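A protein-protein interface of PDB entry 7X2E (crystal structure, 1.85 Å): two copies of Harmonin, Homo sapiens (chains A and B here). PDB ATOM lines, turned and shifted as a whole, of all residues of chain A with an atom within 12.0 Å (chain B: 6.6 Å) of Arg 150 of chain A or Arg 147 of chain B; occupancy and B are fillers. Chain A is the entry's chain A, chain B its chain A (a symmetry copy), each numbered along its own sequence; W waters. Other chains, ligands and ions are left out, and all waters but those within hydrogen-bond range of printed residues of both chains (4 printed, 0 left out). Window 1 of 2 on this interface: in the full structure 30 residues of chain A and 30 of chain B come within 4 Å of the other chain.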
ATOM      1  N   LEU A 139       6.093 -39.454  12.674  1.00  0.00           N
ATOM      2  CA  LEU A 139       7.340 -38.775  13.000  1.00  0.00           C
ATOM      3  C   LEU A 139       8.206 -38.587  11.760  1.00  0.00           C
ATOM      4  O   LEU A 139       8.797 -37.518  11.562  1.00  0.00           O
ATOM      5  CB  LEU A 139       8.089 -39.563  14.075  1.00  0.00           C
ATOM      6  CG  LEU A 139       9.396 -38.968  14.600  1.00  0.00           C
ATOM      7  CD1 LEU A 139       9.131 -37.661  15.331  1.00  0.00           C
ATOM      8  CD2 LEU A 139      10.089 -39.967  15.519  1.00  0.00           C
ATOM      9  N   GLN A 140       8.285 -39.607  10.906  1.00  0.00           N
ATOM     10  CA  GLN A 140       9.075 -39.477   9.689  1.00  0.00           C
ATOM     11  C   GLN A 140       8.464 -38.456   8.738  1.00  0.00           C
ATOM     12  O   GLN A 140       9.189 -37.666   8.121  1.00  0.00           O
ATOM     13  CB  GLN A 140       9.220 -40.835   9.007  1.00  0.00           C
ATOM     14  CG  GLN A 140      10.122 -41.800   9.761  1.00  0.00           C
ATOM     15  CD  GLN A 140      10.022 -43.214   9.233  1.00  0.00           C
ATOM     16  OE1 GLN A 140       9.266 -44.037   9.761  1.00  0.00           O
ATOM     17  NE2 GLN A 140      10.776 -43.504   8.186  1.00  0.00           N
ATOM     18  N   GLU A 141       7.135 -38.451   8.607  1.00  0.00           N
ATOM     19  CA  GLU A 141       6.486 -37.433   7.786  1.00  0.00           C
ATOM     20  C   GLU A 141       6.798 -36.035   8.305  1.00  0.00           C
ATOM     21  O   GLU A 141       7.049 -35.114   7.518  1.00  0.00           O
ATOM     22  CB  GLU A 141       4.976 -37.671   7.750  1.00  0.00           C
ATOM     23  CG  GLU A 141       4.569 -38.943   7.023  1.00  0.00           C
ATOM     24  CD  GLU A 141       3.115 -39.304   7.251  1.00  0.00           C
ATOM     25  OE1 GLU A 141       2.359 -38.440   7.744  1.00  0.00           O
ATOM     26  OE2 GLU A 141       2.728 -40.446   6.934  1.00  0.00           O
ATOM     27  N   GLN A 142       6.805 -35.861   9.630  1.00  0.00           N
ATOM     28  CA  GLN A 142       7.127 -34.558  10.202  1.00  0.00           C
ATOM     29  C   GLN A 142       8.569 -34.168   9.901  1.00  0.00           C
ATOM     30  O   GLN A 142       8.858 -32.998   9.627  1.00  0.00           O
ATOM     31  CB  GLN A 142       6.879 -34.565  11.711  1.00  0.00           C
ATOM     32  CG  GLN A 142       5.409 -34.609  12.097  1.00  0.00           C
ATOM     33  CD  GLN A 142       5.201 -35.005  13.545  1.00  0.00           C
ATOM     34  OE1 GLN A 142       6.157 -35.278  14.269  1.00  0.00           O
ATOM     35  NE2 GLN A 142       3.944 -35.027  13.977  1.00  0.00           N
ATOM     36  N   GLN A 143       9.491 -35.135   9.947  1.00  0.00           N
ATOM     37  CA  GLN A 143      10.881 -34.834   9.617  1.00  0.00           C
ATOM     38  C   GLN A 143      11.034 -34.439   8.153  1.00  0.00           C
ATOM     39  O   GLN A 143      11.781 -33.507   7.835  1.00  0.00           O
ATOM     40  CB  GLN A 143      11.785 -36.023   9.941  1.00  0.00           C
ATOM     41  CG  GLN A 143      11.738 -36.505  11.388  1.00  0.00           C
ATOM     42  CD  GLN A 143      11.474 -35.392  12.387  1.00  0.00           C
ATOM     43  OE1 GLN A 143      12.285 -34.483  12.556  1.00  0.00           O
ATOM     44  NE2 GLN A 143      10.339 -35.471  13.065  1.00  0.00           N
ATOM     45  N   GLU A 144      10.340 -35.135   7.246  1.00  0.00           N
ATOM     46  CA  GLU A 144      10.419 -34.779   5.830  1.00  0.00           C
ATOM     47  C   GLU A 144       9.909 -33.364   5.580  1.00  0.00           C
ATOM     48  O   GLU A 144      10.518 -32.604   4.815  1.00  0.00           O
ATOM     49  CB  GLU A 144       9.642 -35.791   4.984  1.00  0.00           C
ATOM     50  CG  GLU A 144      10.096 -37.228   5.178  1.00  0.00           C
ATOM     51  CD  GLU A 144       9.115 -38.245   4.622  1.00  0.00           C
ATOM     52  OE1 GLU A 144       7.959 -37.871   4.327  1.00  0.00           O
ATOM     53  OE2 GLU A 144       9.499 -39.427   4.494  1.00  0.00           O
ATOM     54  N   MET A 145       8.794 -32.991   6.214  1.00  0.00           N
ATOM     55  CA  MET A 145       8.265 -31.637   6.055  1.00  0.00           C
ATOM     56  C   MET A 145       9.252 -30.599   6.566  1.00  0.00           C
ATOM     57  O   MET A 145       9.544 -29.606   5.886  1.00  0.00           O
ATOM     58  CB  MET A 145       6.937 -31.492   6.799  1.00  0.00           C
ATOM     59  CG  MET A 145       5.817 -32.344   6.274  1.00  0.00           C
ATOM     60  SD  MET A 145       4.241 -31.966   7.065  1.00  0.00           S
ATOM     61  CE  MET A 145       4.371 -30.189   7.241  1.00  0.00           C
ATOM     62  N   GLU A 146       9.769 -30.810   7.776  1.00  0.00           N
ATOM     63  CA  GLU A 146      10.619 -29.803   8.399  1.00  0.00           C
ATOM     64  C   GLU A 146      11.960 -29.686   7.683  1.00  0.00           C
ATOM     65  O   GLU A 146      12.504 -28.583   7.560  1.00  0.00           O
ATOM     66  CB  GLU A 146      10.814 -30.129   9.880  1.00  0.00           C
ATOM     67  CG  GLU A 146      11.539 -29.051  10.677  1.00  0.00           C
ATOM     68  CD  GLU A 146      10.712 -27.793  10.893  1.00  0.00           C
ATOM     69  OE1 GLU A 146      11.238 -26.842  11.509  1.00  0.00           O
ATOM     70  OE2 GLU A 146       9.539 -27.751  10.463  1.00  0.00           O
ATOM     71  N   ARG A 147      12.510 -30.803   7.193  1.00  0.00           N
ATOM     72  CA  ARG A 147      13.790 -30.711   6.494  1.00  0.00           C
ATOM     73  C   ARG A 147      13.647 -30.019   5.142  1.00  0.00           C
ATOM     74  O   ARG A 147      14.563 -29.306   4.716  1.00  0.00           O
ATOM     75  CB  ARG A 147      14.426 -32.096   6.332  1.00  0.00           C
ATOM     76  CG  ARG A 147      14.751 -32.781   7.661  1.00  0.00           C
ATOM     77  CD  ARG A 147      15.468 -34.114   7.466  1.00  0.00           C
ATOM     78  NE  ARG A 147      16.862 -33.936   7.069  1.00  0.00           N
ATOM     79  CZ  ARG A 147      17.344 -34.202   5.859  1.00  0.00           C
ATOM     80  NH1 ARG A 147      18.628 -34.005   5.603  1.00  0.00           N
ATOM     81  NH2 ARG A 147      16.547 -34.671   4.910  1.00  0.00           N
ATOM     82  N   GLN A 148      12.512 -30.194   4.461  1.00  0.00           N
ATOM     83  CA  GLN A 148      12.301 -29.460   3.217  1.00  0.00           C
ATOM     84  C   GLN A 148      12.085 -27.977   3.486  1.00  0.00           C
ATOM     85  O   GLN A 148      12.616 -27.125   2.763  1.00  0.00           O
ATOM     86  CB  GLN A 148      11.116 -30.045   2.445  1.00  0.00           C
ATOM     87  CG  GLN A 148      10.860 -29.382   1.088  1.00  0.00           C
ATOM     88  CD  GLN A 148      12.103 -29.302   0.214  1.00  0.00           C
ATOM     89  OE1 GLN A 148      12.900 -30.237   0.160  1.00  0.00           O
ATOM     90  NE2 GLN A 148      12.266 -28.181  -0.483  1.00  0.00           N
ATOM     91  N   ARG A 149      11.306 -27.653   4.521  1.00  0.00           N
ATOM     92  CA  ARG A 149      11.093 -26.254   4.885  1.00  0.00           C
ATOM     93  C   ARG A 149      12.409 -25.563   5.224  1.00  0.00           C
ATOM     94  O   ARG A 149      12.654 -24.427   4.801  1.00  0.00           O
ATOM     95  CB  ARG A 149      10.126 -26.168   6.066  1.00  0.00           C
ATOM     96  CG  ARG A 149       9.759 -24.753   6.475  1.00  0.00           C
ATOM     97  CD  ARG A 149       8.876 -24.748   7.717  1.00  0.00           C
ATOM     98  NE  ARG A 149       9.649 -24.897   8.949  1.00  0.00           N
ATOM     99  CZ  ARG A 149      10.147 -23.883   9.651  1.00  0.00           C
ATOM    100  NH1 ARG A 149       9.957 -22.636   9.245  1.00  0.00           N
ATOM    101  NH2 ARG A 149      10.837 -24.117  10.761  1.00  0.00           N
ATOM    102  N   ARG A 150      13.272 -26.236   5.980  1.00  0.00           N
ATOM    103  CA  ARG A 150      14.532 -25.622   6.379  1.00  0.00           C
ATOM    104  C   ARG A 150      15.544 -25.612   5.242  1.00  0.00           C
ATOM    105  O   ARG A 150      16.420 -24.741   5.206  1.00  0.00           O
ATOM    106  CB  ARG A 150      15.079 -26.345   7.606  1.00  0.00           C
ATOM    107  CG  ARG A 150      14.217 -26.103   8.832  1.00  0.00           C
ATOM    108  CD  ARG A 150      14.733 -26.828  10.052  1.00  0.00           C
ATOM    109  NE  ARG A 150      13.865 -26.596  11.201  1.00  0.00           N
ATOM    110  CZ  ARG A 150      14.024 -25.595  12.061  1.00  0.00           C
ATOM    111  NH1 ARG A 150      15.016 -24.732  11.898  1.00  0.00           N
ATOM    112  NH2 ARG A 150      13.189 -25.455  13.081  1.00  0.00           N
ATOM    113  N   LYS A 151      15.444 -26.562   4.311  1.00  0.00           N
ATOM    114  CA  LYS A 151      16.241 -26.479   3.091  1.00  0.00           C
ATOM    115  C   LYS A 151      15.887 -25.227   2.300  1.00  0.00           C
ATOM    116  O   LYS A 151      16.772 -24.547   1.764  1.00  0.00           O
ATOM    117  CB  LYS A 151      16.025 -27.728   2.240  1.00  0.00           C
ATOM    118  CG  LYS A 151      16.705 -27.681   0.881  1.00  0.00           C
ATOM    119  CD  LYS A 151      16.279 -28.857   0.015  1.00  0.00           C
ATOM    120  CE  LYS A 151      17.406 -29.309  -0.897  1.00  0.00           C
ATOM    121  NZ  LYS A 151      17.184 -30.693  -1.401  1.00  0.00           N
ATOM    122  N   GLU A 152      14.594 -24.907   2.222  1.00  0.00           N
ATOM    123  CA  GLU A 152      14.161 -23.717   1.497  1.00  0.00           C
ATOM    124  C   GLU A 152      14.634 -22.446   2.195  1.00  0.00           C
ATOM    125  O   GLU A 152      15.058 -21.489   1.534  1.00  0.00           O
ATOM    126  CB  GLU A 152      12.639 -23.732   1.357  1.00  0.00           C
ATOM    127  CG  GLU A 152      12.147 -24.643   0.241  1.00  0.00           C
ATOM    128  CD  GLU A 152      10.671 -24.970   0.348  1.00  0.00           C
ATOM    129  OE1 GLU A 152      10.220 -25.904  -0.348  1.00  0.00           O
ATOM    130  OE2 GLU A 152       9.960 -24.296   1.126  1.00  0.00           O
ATOM    131  N   ILE A 153      14.576 -22.424   3.529  1.00  0.00           N
ATOM    132  CA  ILE A 153      15.092 -21.293   4.296  1.00  0.00           C
ATOM    133  C   ILE A 153      16.582 -21.108   4.041  1.00  0.00           C
ATOM    134  O   ILE A 153      17.065 -19.979   3.875  1.00  0.00           O
ATOM    135  CB  ILE A 153      14.797 -21.492   5.796  1.00  0.00           C
ATOM    136  CG1 ILE A 153      13.298 -21.345   6.066  1.00  0.00           C
ATOM    137  CG2 ILE A 153      15.603 -20.515   6.644  1.00  0.00           C
ATOM    138  CD1 ILE A 153      12.859 -21.902   7.399  1.00  0.00           C
ATOM    139  N   ALA A 154      17.332 -22.211   3.993  1.00  0.00           N
ATOM    140  CA  ALA A 154      18.777 -22.116   3.806  1.00  0.00           C
ATOM    141  C   ALA A 154      19.128 -21.603   2.414  1.00  0.00           C
ATOM    142  O   ALA A 154      20.017 -20.755   2.268  1.00  0.00           O
ATOM    143  CB  ALA A 154      19.425 -23.478   4.060  1.00  0.00           C
ATOM    144  N   GLN A 155      18.449 -22.101   1.378  1.00  0.00           N
ATOM    145  CA  GLN A 155      18.773 -21.679   0.019  1.00  0.00           C
ATOM    146  C   GLN A 155      18.414 -20.215  -0.204  1.00  0.00           C
ATOM    147  O   GLN A 155      19.117 -19.500  -0.927  1.00  0.00           O
ATOM    148  CB  GLN A 155      18.058 -22.568  -0.999  1.00  0.00           C
ATOM    149  CG  GLN A 155      18.701 -22.546  -2.377  1.00  0.00           C
ATOM    150  CD  GLN A 155      17.756 -22.993  -3.474  1.00  0.00           C
ATOM    151  OE1 GLN A 155      17.089 -24.022  -3.358  1.00  0.00           O
ATOM    152  NE2 GLN A 155      17.693 -22.217  -4.552  1.00  0.00           N
ATOM    153  N   LYS A 156      17.319 -19.756   0.404  1.00  0.00           N
ATOM    154  CA  LYS A 156      16.969 -18.340   0.349  1.00  0.00           C
ATOM    155  C   LYS A 156      18.061 -17.484   0.975  1.00  0.00           C
ATOM    156  O   LYS A 156      18.474 -16.465   0.407  1.00  0.00           O
ATOM    157  CB  LYS A 156      15.635 -18.109   1.056  1.00  0.00           C
ATOM    158  CG  LYS A 156      15.239 -16.650   1.196  1.00  0.00           C
ATOM    159  CD  LYS A 156      13.778 -16.518   1.589  1.00  0.00           C
ATOM    160  CE  LYS A 156      13.383 -15.062   1.760  1.00  0.00           C
ATOM    161  NZ  LYS A 156      12.132 -14.913   2.559  1.00  0.00           N
ATOM    162  N   ALA A 157      18.541 -17.888   2.155  1.00  0.00           N
ATOM    163  CA  ALA A 157      19.607 -17.148   2.823  1.00  0.00           C
ATOM    164  C   ALA A 157      20.889 -17.157   2.002  1.00  0.00           C
ATOM    165  O   ALA A 157      21.614 -16.157   1.959  1.00  0.00           O
ATOM    166  CB  ALA A 157      19.858 -17.736   4.214  1.00  0.00           C
ATOM    167  N   ALA A 158      21.184 -18.279   1.339  1.00  0.00           N
ATOM    168  CA  ALA A 158      22.399 -18.365   0.535  1.00  0.00           C
ATOM    169  C   ALA A 158      22.342 -17.412  -0.654  1.00  0.00           C
ATOM    170  O   ALA A 158      23.307 -16.694  -0.935  1.00  0.00           O
ATOM    171  CB  ALA A 158      22.621 -19.804   0.063  1.00  0.00           C
ATOM    172  N   GLU A 159      21.214 -17.386  -1.368  1.00  0.00           N
ATOM    173  CA  GLU A 159      21.160 -16.519  -2.540  1.00  0.00           C
ATOM    174  C   GLU A 159      21.069 -15.051  -2.148  1.00  0.00           C
ATOM    175  O   GLU A 159      21.574 -14.191  -2.878  1.00  0.00           O
ATOM    176  CB  GLU A 159      20.007 -16.909  -3.468  1.00  0.00           C
ATOM    177  CG  GLU A 159      18.608 -16.682  -2.941  1.00  0.00           C
ATOM    178  CD  GLU A 159      17.554 -17.204  -3.905  1.00  0.00           C
ATOM    179  OE1 GLU A 159      17.096 -16.420  -4.765  1.00  0.00           O
ATOM    180  OE2 GLU A 159      17.200 -18.398  -3.818  1.00  0.00           O
ATOM    181  N   GLU A 160      20.447 -14.738  -1.007  1.00  0.00           N
ATOM    182  CA  GLU A 160      20.507 -13.368  -0.508  1.00  0.00           C
ATOM    183  C   GLU A 160      21.948 -12.955  -0.239  1.00  0.00           C
ATOM    184  O   GLU A 160      22.365 -11.850  -0.605  1.00  0.00           O
ATOM    185  CB  GLU A 160      19.662 -13.215   0.759  1.00  0.00           C
ATOM    186  CG  GLU A 160      18.158 -13.153   0.511  1.00  0.00           C
ATOM    187  CD  GLU A 160      17.354 -13.055   1.799  1.00  0.00           C
ATOM    188  OE1 GLU A 160      17.911 -13.325   2.886  1.00  0.00           O
ATOM    189  OE2 GLU A 160      16.159 -12.700   1.720  1.00  0.00           O
ATOM    190  N   GLN B 142      22.291 -22.947  11.368  1.00  0.00           N
ATOM    191  CA  GLN B 142      21.201 -23.513  12.155  1.00  0.00           C
ATOM    192  C   GLN B 142      20.392 -24.509  11.336  1.00  0.00           C
ATOM    193  O   GLN B 142      19.965 -25.548  11.855  1.00  0.00           O
ATOM    194  CB  GLN B 142      20.299 -22.399  12.688  1.00  0.00           C
ATOM    195  CG  GLN B 142      20.934 -21.554  13.781  1.00  0.00           C
ATOM    196  CD  GLN B 142      20.197 -20.250  14.009  1.00  0.00           C
ATOM    197  OE1 GLN B 142      19.215 -19.952  13.331  1.00  0.00           O
ATOM    198  NE2 GLN B 142      20.664 -19.469  14.978  1.00  0.00           N
ATOM    199  N   GLN B 143      20.168 -24.213  10.052  1.00  0.00           N
ATOM    200  CA  GLN B 143      19.443 -25.154   9.202  1.00  0.00           C
ATOM    201  C   GLN B 143      20.226 -26.447   9.008  1.00  0.00           C
ATOM    202  O   GLN B 143      19.643 -27.537   9.035  1.00  0.00           O
ATOM    203  CB  GLN B 143      19.120 -24.523   7.847  1.00  0.00           C
ATOM    204  CG  GLN B 143      18.319 -23.226   7.905  1.00  0.00           C
ATOM    205  CD  GLN B 143      17.357 -23.162   9.078  1.00  0.00           C
ATOM    206  OE1 GLN B 143      16.404 -23.933   9.163  1.00  0.00           O
ATOM    207  NE2 GLN B 143      17.599 -22.225   9.984  1.00  0.00           N
ATOM    208  N   GLU B 144      21.545 -26.351   8.806  1.00  0.00           N
ATOM    209  CA  GLU B 144      22.353 -27.559   8.650  1.00  0.00           C
ATOM    210  C   GLU B 144      22.300 -28.434   9.898  1.00  0.00           C
ATOM    211  O   GLU B 144      22.179 -29.662   9.798  1.00  0.00           O
ATOM    212  CB  GLU B 144      23.799 -27.190   8.309  1.00  0.00           C
ATOM    213  CG  GLU B 144      23.933 -26.318   7.072  1.00  0.00           C
ATOM    214  CD  GLU B 144      25.302 -25.674   6.941  1.00  0.00           C
ATOM    215  OE1 GLU B 144      26.067 -25.672   7.930  1.00  0.00           O
ATOM    216  OE2 GLU B 144      25.608 -25.155   5.846  1.00  0.00           O
ATOM    217  N   MET B 145      22.390 -27.822  11.082  1.00  0.00           N
ATOM    218  CA  MET B 145      22.308 -28.589  12.324  1.00  0.00           C
ATOM    219  C   MET B 145      20.959 -29.280  12.454  1.00  0.00           C
ATOM    220  O   MET B 145      20.882 -30.479  12.753  1.00  0.00           O
ATOM    221  CB  MET B 145      22.535 -27.678  13.530  1.00  0.00           C
ATOM    222  CG  MET B 145      23.904 -27.065  13.615  1.00  0.00           C
ATOM    223  SD  MET B 145      24.161 -26.175  15.163  1.00  0.00           S
ATOM    224  CE  MET B 145      23.285 -27.236  16.308  1.00  0.00           C
ATOM    225  N   GLU B 146      19.879 -28.528  12.242  1.00  0.00           N
ATOM    226  CA  GLU B 146      18.547 -29.072  12.475  1.00  0.00           C
ATOM    227  C   GLU B 146      18.192 -30.136  11.441  1.00  0.00           C
ATOM    228  O   GLU B 146      17.531 -31.127  11.773  1.00  0.00           O
ATOM    229  CB  GLU B 146      17.516 -27.943  12.476  1.00  0.00           C
ATOM    230  CG  GLU B 146      16.110 -28.367  12.885  1.00  0.00           C
ATOM    231  CD  GLU B 146      15.983 -28.708  14.362  1.00  0.00           C
ATOM    232  OE1 GLU B 146      14.873 -29.099  14.781  1.00  0.00           O
ATOM    233  OE2 GLU B 146      16.978 -28.579  15.107  1.00  0.00           O
ATOM    234  N   ARG B 147      18.626 -29.964  10.188  1.00  0.00           N
ATOM    235  CA  ARG B 147      18.305 -30.978   9.185  1.00  0.00           C
ATOM    236  C   ARG B 147      19.076 -32.272   9.425  1.00  0.00           C
ATOM    237  O   ARG B 147      18.549 -33.359   9.160  1.00  0.00           O
ATOM    238  CB  ARG B 147      18.559 -30.448   7.770  1.00  0.00           C
ATOM    239  CG  ARG B 147      17.692 -29.242   7.402  1.00  0.00           C
ATOM    240  CD  ARG B 147      17.900 -28.797   5.957  1.00  0.00           C
ATOM    241  NE  ARG B 147      17.266 -29.706   5.005  1.00  0.00           N
ATOM    242  CZ  ARG B 147      17.923 -30.533   4.197  1.00  0.00           C
ATOM    243  NH1 ARG B 147      17.250 -31.317   3.370  1.00  0.00           N
ATOM    244  NH2 ARG B 147      19.247 -30.571   4.211  1.00  0.00           N
ATOM    245  N   GLN B 148      20.305 -32.189   9.937  1.00  0.00           N
ATOM    246  CA  GLN B 148      21.026 -33.412  10.279  1.00  0.00           C
ATOM    247  C   GLN B 148      20.406 -34.092  11.492  1.00  0.00           C
ATOM    248  O   GLN B 148      20.267 -35.321  11.519  1.00  0.00           O
ATOM    249  CB  GLN B 148      22.505 -33.109  10.529  1.00  0.00           C
ATOM    250  CG  GLN B 148      23.358 -34.347  10.827  1.00  0.00           C
ATOM    251  CD  GLN B 148      23.188 -35.456   9.800  1.00  0.00           C
ATOM    252  OE1 GLN B 148      23.097 -35.201   8.600  1.00  0.00           O
ATOM    253  NE2 GLN B 148      23.151 -36.700  10.272  1.00  0.00           N
ATOM    254  N   ARG B 149      20.029 -33.307  12.505  1.00  0.00           N
ATOM    255  CA  ARG B 149      19.373 -33.870  13.682  1.00  0.00           C
ATOM    256  C   ARG B 149      18.078 -34.581  13.307  1.00  0.00           C
ATOM    257  O   ARG B 149      17.795 -35.681  13.798  1.00  0.00           O
ATOM    258  CB  ARG B 149      19.100 -32.764  14.701  1.00  0.00           C
ATOM    259  CG  ARG B 149      18.499 -33.250  16.008  1.00  0.00           C
ATOM    260  CD  ARG B 149      18.162 -32.083  16.928  1.00  0.00           C
ATOM    261  NE  ARG B 149      16.888 -31.453  16.584  1.00  0.00           N
ATOM    262  CZ  ARG B 149      15.711 -31.815  17.086  1.00  0.00           C
ATOM    263  NH1 ARG B 149      15.638 -32.808  17.960  1.00  0.00           N
ATOM    264  NH2 ARG B 149      14.606 -31.182  16.714  1.00  0.00           N
ATOM    265  N   ARG B 150      17.282 -33.972  12.433  1.00  0.00           N
ATOM    266  CA  ARG B 150      16.007 -34.571  12.060  1.00  0.00           C
ATOM    267  C   ARG B 150      16.186 -35.726  11.084  1.00  0.00           C
ATOM    268  O   ARG B 150      15.351 -36.637  11.048  1.00  0.00           O
ATOM    269  CB  ARG B 150      15.091 -33.495  11.487  1.00  0.00           C
ATOM    270  CG  ARG B 150      14.663 -32.497  12.548  1.00  0.00           C
ATOM    271  CD  ARG B 150      13.772 -31.412  11.993  1.00  0.00           C
ATOM    272  NE  ARG B 150      13.404 -30.458  13.034  1.00  0.00           N
ATOM    273  CZ  ARG B 150      12.327 -30.576  13.803  1.00  0.00           C
ATOM    274  NH1 ARG B 150      11.513 -31.611  13.650  1.00  0.00           N
ATOM    275  NH2 ARG B 150      12.066 -29.663  14.727  1.00  0.00           N
ATOM    276  N   LYS B 151      17.259 -35.711  10.291  1.00  0.00           N
ATOM    277  CA  LYS B 151      17.599 -36.885   9.495  1.00  0.00           C
ATOM    278  C   LYS B 151      17.892 -38.079  10.393  1.00  0.00           C
ATOM    279  O   LYS B 151      17.474 -39.208  10.103  1.00  0.00           O
ATOM    280  CB  LYS B 151      18.799 -36.582   8.601  1.00  0.00           C
ATOM    281  CG  LYS B 151      19.321 -37.783   7.830  1.00  0.00           C
ATOM    282  CD  LYS B 151      20.631 -37.456   7.128  1.00  0.00           C
ATOM    283  CE  LYS B 151      20.759 -38.209   5.816  1.00  0.00           C
ATOM    284  NZ  LYS B 151      21.770 -37.584   4.919  1.00  0.00           N
ATOM    285  N   GLU B 152      18.608 -37.845  11.496  1.00  0.00           N
ATOM    286  CA  GLU B 152      18.926 -38.925  12.424  1.00  0.00           C
ATOM    287  C   GLU B 152      17.669 -39.443  13.115  1.00  0.00           C
ATOM    288  O   GLU B 152      17.513 -40.656  13.303  1.00  0.00           O
ATOM    289  CB  GLU B 152      19.951 -38.432  13.446  1.00  0.00           C
ATOM    290  CG  GLU B 152      21.375 -38.417  12.908  1.00  0.00           C
ATOM    291  CD  GLU B 152      22.318 -37.577  13.748  1.00  0.00           C
ATOM    292  OE1 GLU B 152      23.432 -37.281  13.267  1.00  0.00           O
ATOM    293  OE2 GLU B 152      21.948 -37.213  14.886  1.00  0.00           O
HETATM  294  O   HOH W   1      21.226 -33.373   6.973  1.00  0.00           O
HETATM  295  O   HOH W   2      10.485 -26.643  14.466  1.00  0.00           O
HETATM  296  O   HOH W   3      13.183 -26.951  16.154  1.00  0.00           O
HETATM  297  O   HOH W   4      14.478 -31.783   2.306  1.00  0.00           O
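NE of Arg 150 of chain B touches CG of Glu 146 of chain A, at 3.3 Å. CB of Arg 150 of chain B touches CG of Arg 147 of chain A, 3.9 Å away. NE of Arg 147 of chain A touches CB of Lys 151 of chain B (3.6 Å). CG of Glu 146 of chain B touches NE of Arg 150 of chain A, 3.3 Å away. Arg 147 of chain B touches Arg 150 of chain A. NE of Arg 147 of chain B touches CB of Lys 151 of chain A, 3.6 Å away. Gln 143 of chain B touches Ala 154 of chain A (CB to CB, 3.9 Å).
The guanidinium group (NH1) of Arg 150 of chain A sits close to the side-chain amide oxygen (OE1) of Gln 143 of chain B (3.2 Å). The side-chain amide oxygen (OE1) of Gln 143 of chain A lies close to the guanidinium group (NH1) of Arg 150 of chain B, at 3.2 Å. O of Arg 147 of chain B lies within hydrogen-bond range of NE of Arg 147 of chain A.
Glu 146 of chain A touches Arg 150 of chain B, and with the chains exchanged Arg 150 of chain A touches Glu 146 of chain B. Arg 147 of chain A touches its own counterpart, Arg 147 of chain B. Arg 147 of chain A touches Arg 150 of chain B, and with the chains exchanged Arg 150 of chain A touches Arg 147 of chain B. Arg 147 of chain A touches Lys 151 of chain B, and with the chains exchanged Lys 151 of chain A touches Arg 147 of chain B. Of the 10 pairs that touch across the chains among the printed residues, 9 have their exchanged pair printed and touching as well.
Water W1 lies within hydrogen-bond range of NH1 of Arg 147 of chain A, OE1 of Gln 148 of chain B and O of Arg 147 of chain B. Water W4 lies within hydrogen-bond range of the guanidinium group (NH1) of Arg 147 of chain B (3.0 Å), the side-chain amide oxygen (OE1) of Gln 148 of chain A (3.1 Å) and the backbone carbonyl oxygen (O) of Arg 147 of chain A (3.5 Å). Water W2 lies within hydrogen-bond range of OE1 of Glu 146 of chain A (3.1 Å), NH2 of Arg 150 of chain A (3.3 Å) and NH2 of Arg 150 of chain B (3.4 Å). Water W3 lies within hydrogen-bond range of the side-chain carboxylate (OE1) of Glu 146 of chain B, the guanidinium group (NH2) of Arg 150 of chain B and the guanidinium group (NH2) of Arg 150 of chain A.
Of the printed residues of chain B, Gln 143 of chain A touches Arg 150. Printed residues of chain B within 4 Å of Glu 146 of chain A: Arg 150. Printed residues of chain B within 4 Å of Arg 147 of chain A: Arg 147, Arg 150 and Lys 151. Arg 150 of chain A touches just these residues of chain B: Gln 143 (3.1 Å), Glu 146 (3.3 Å) and Arg 147 (3.9 Å). Arg 147 of chain B touches just these residues of chain A: Arg 147, Arg 150 and Lys 151. No residue of chain A comes within 4 Å of Gln 148 of chain B. Arg 150 of chain B touches just these residues of chain A: Gln 143, Glu 146 and Arg 147. Lys 151 of chain B touches just one residue of chain A: Arg 147. The nearest residue of chain B that does not touch Arg 150 of chain A is Arg 150 of chain B (4.3 Å).
O of Leu 139 of chain A sits at hydrogen-bond distance from NE2 of Gln 143 of chain A (3.0 Å). NH2 of Arg 149 of chain B is in salt-bridge range of OE1 of Glu 146 of chain B (2.9 Å). The side-chain carboxylate of Glu 146 of chain A lies within salt-bridge range of the guanidinium group of Arg 150 of chain A (2.7 Å). OE1 of Glu 146 of chain A lies within salt-bridge range of NH2 of Arg 149 of chain A, 2.9 Å away. OE1 of Glu 146 of chain B lies within salt-bridge range of NE of Arg 150 of chain B, 2.7 Å away.
Among the printed residues, 10 pairs touch across the chains.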
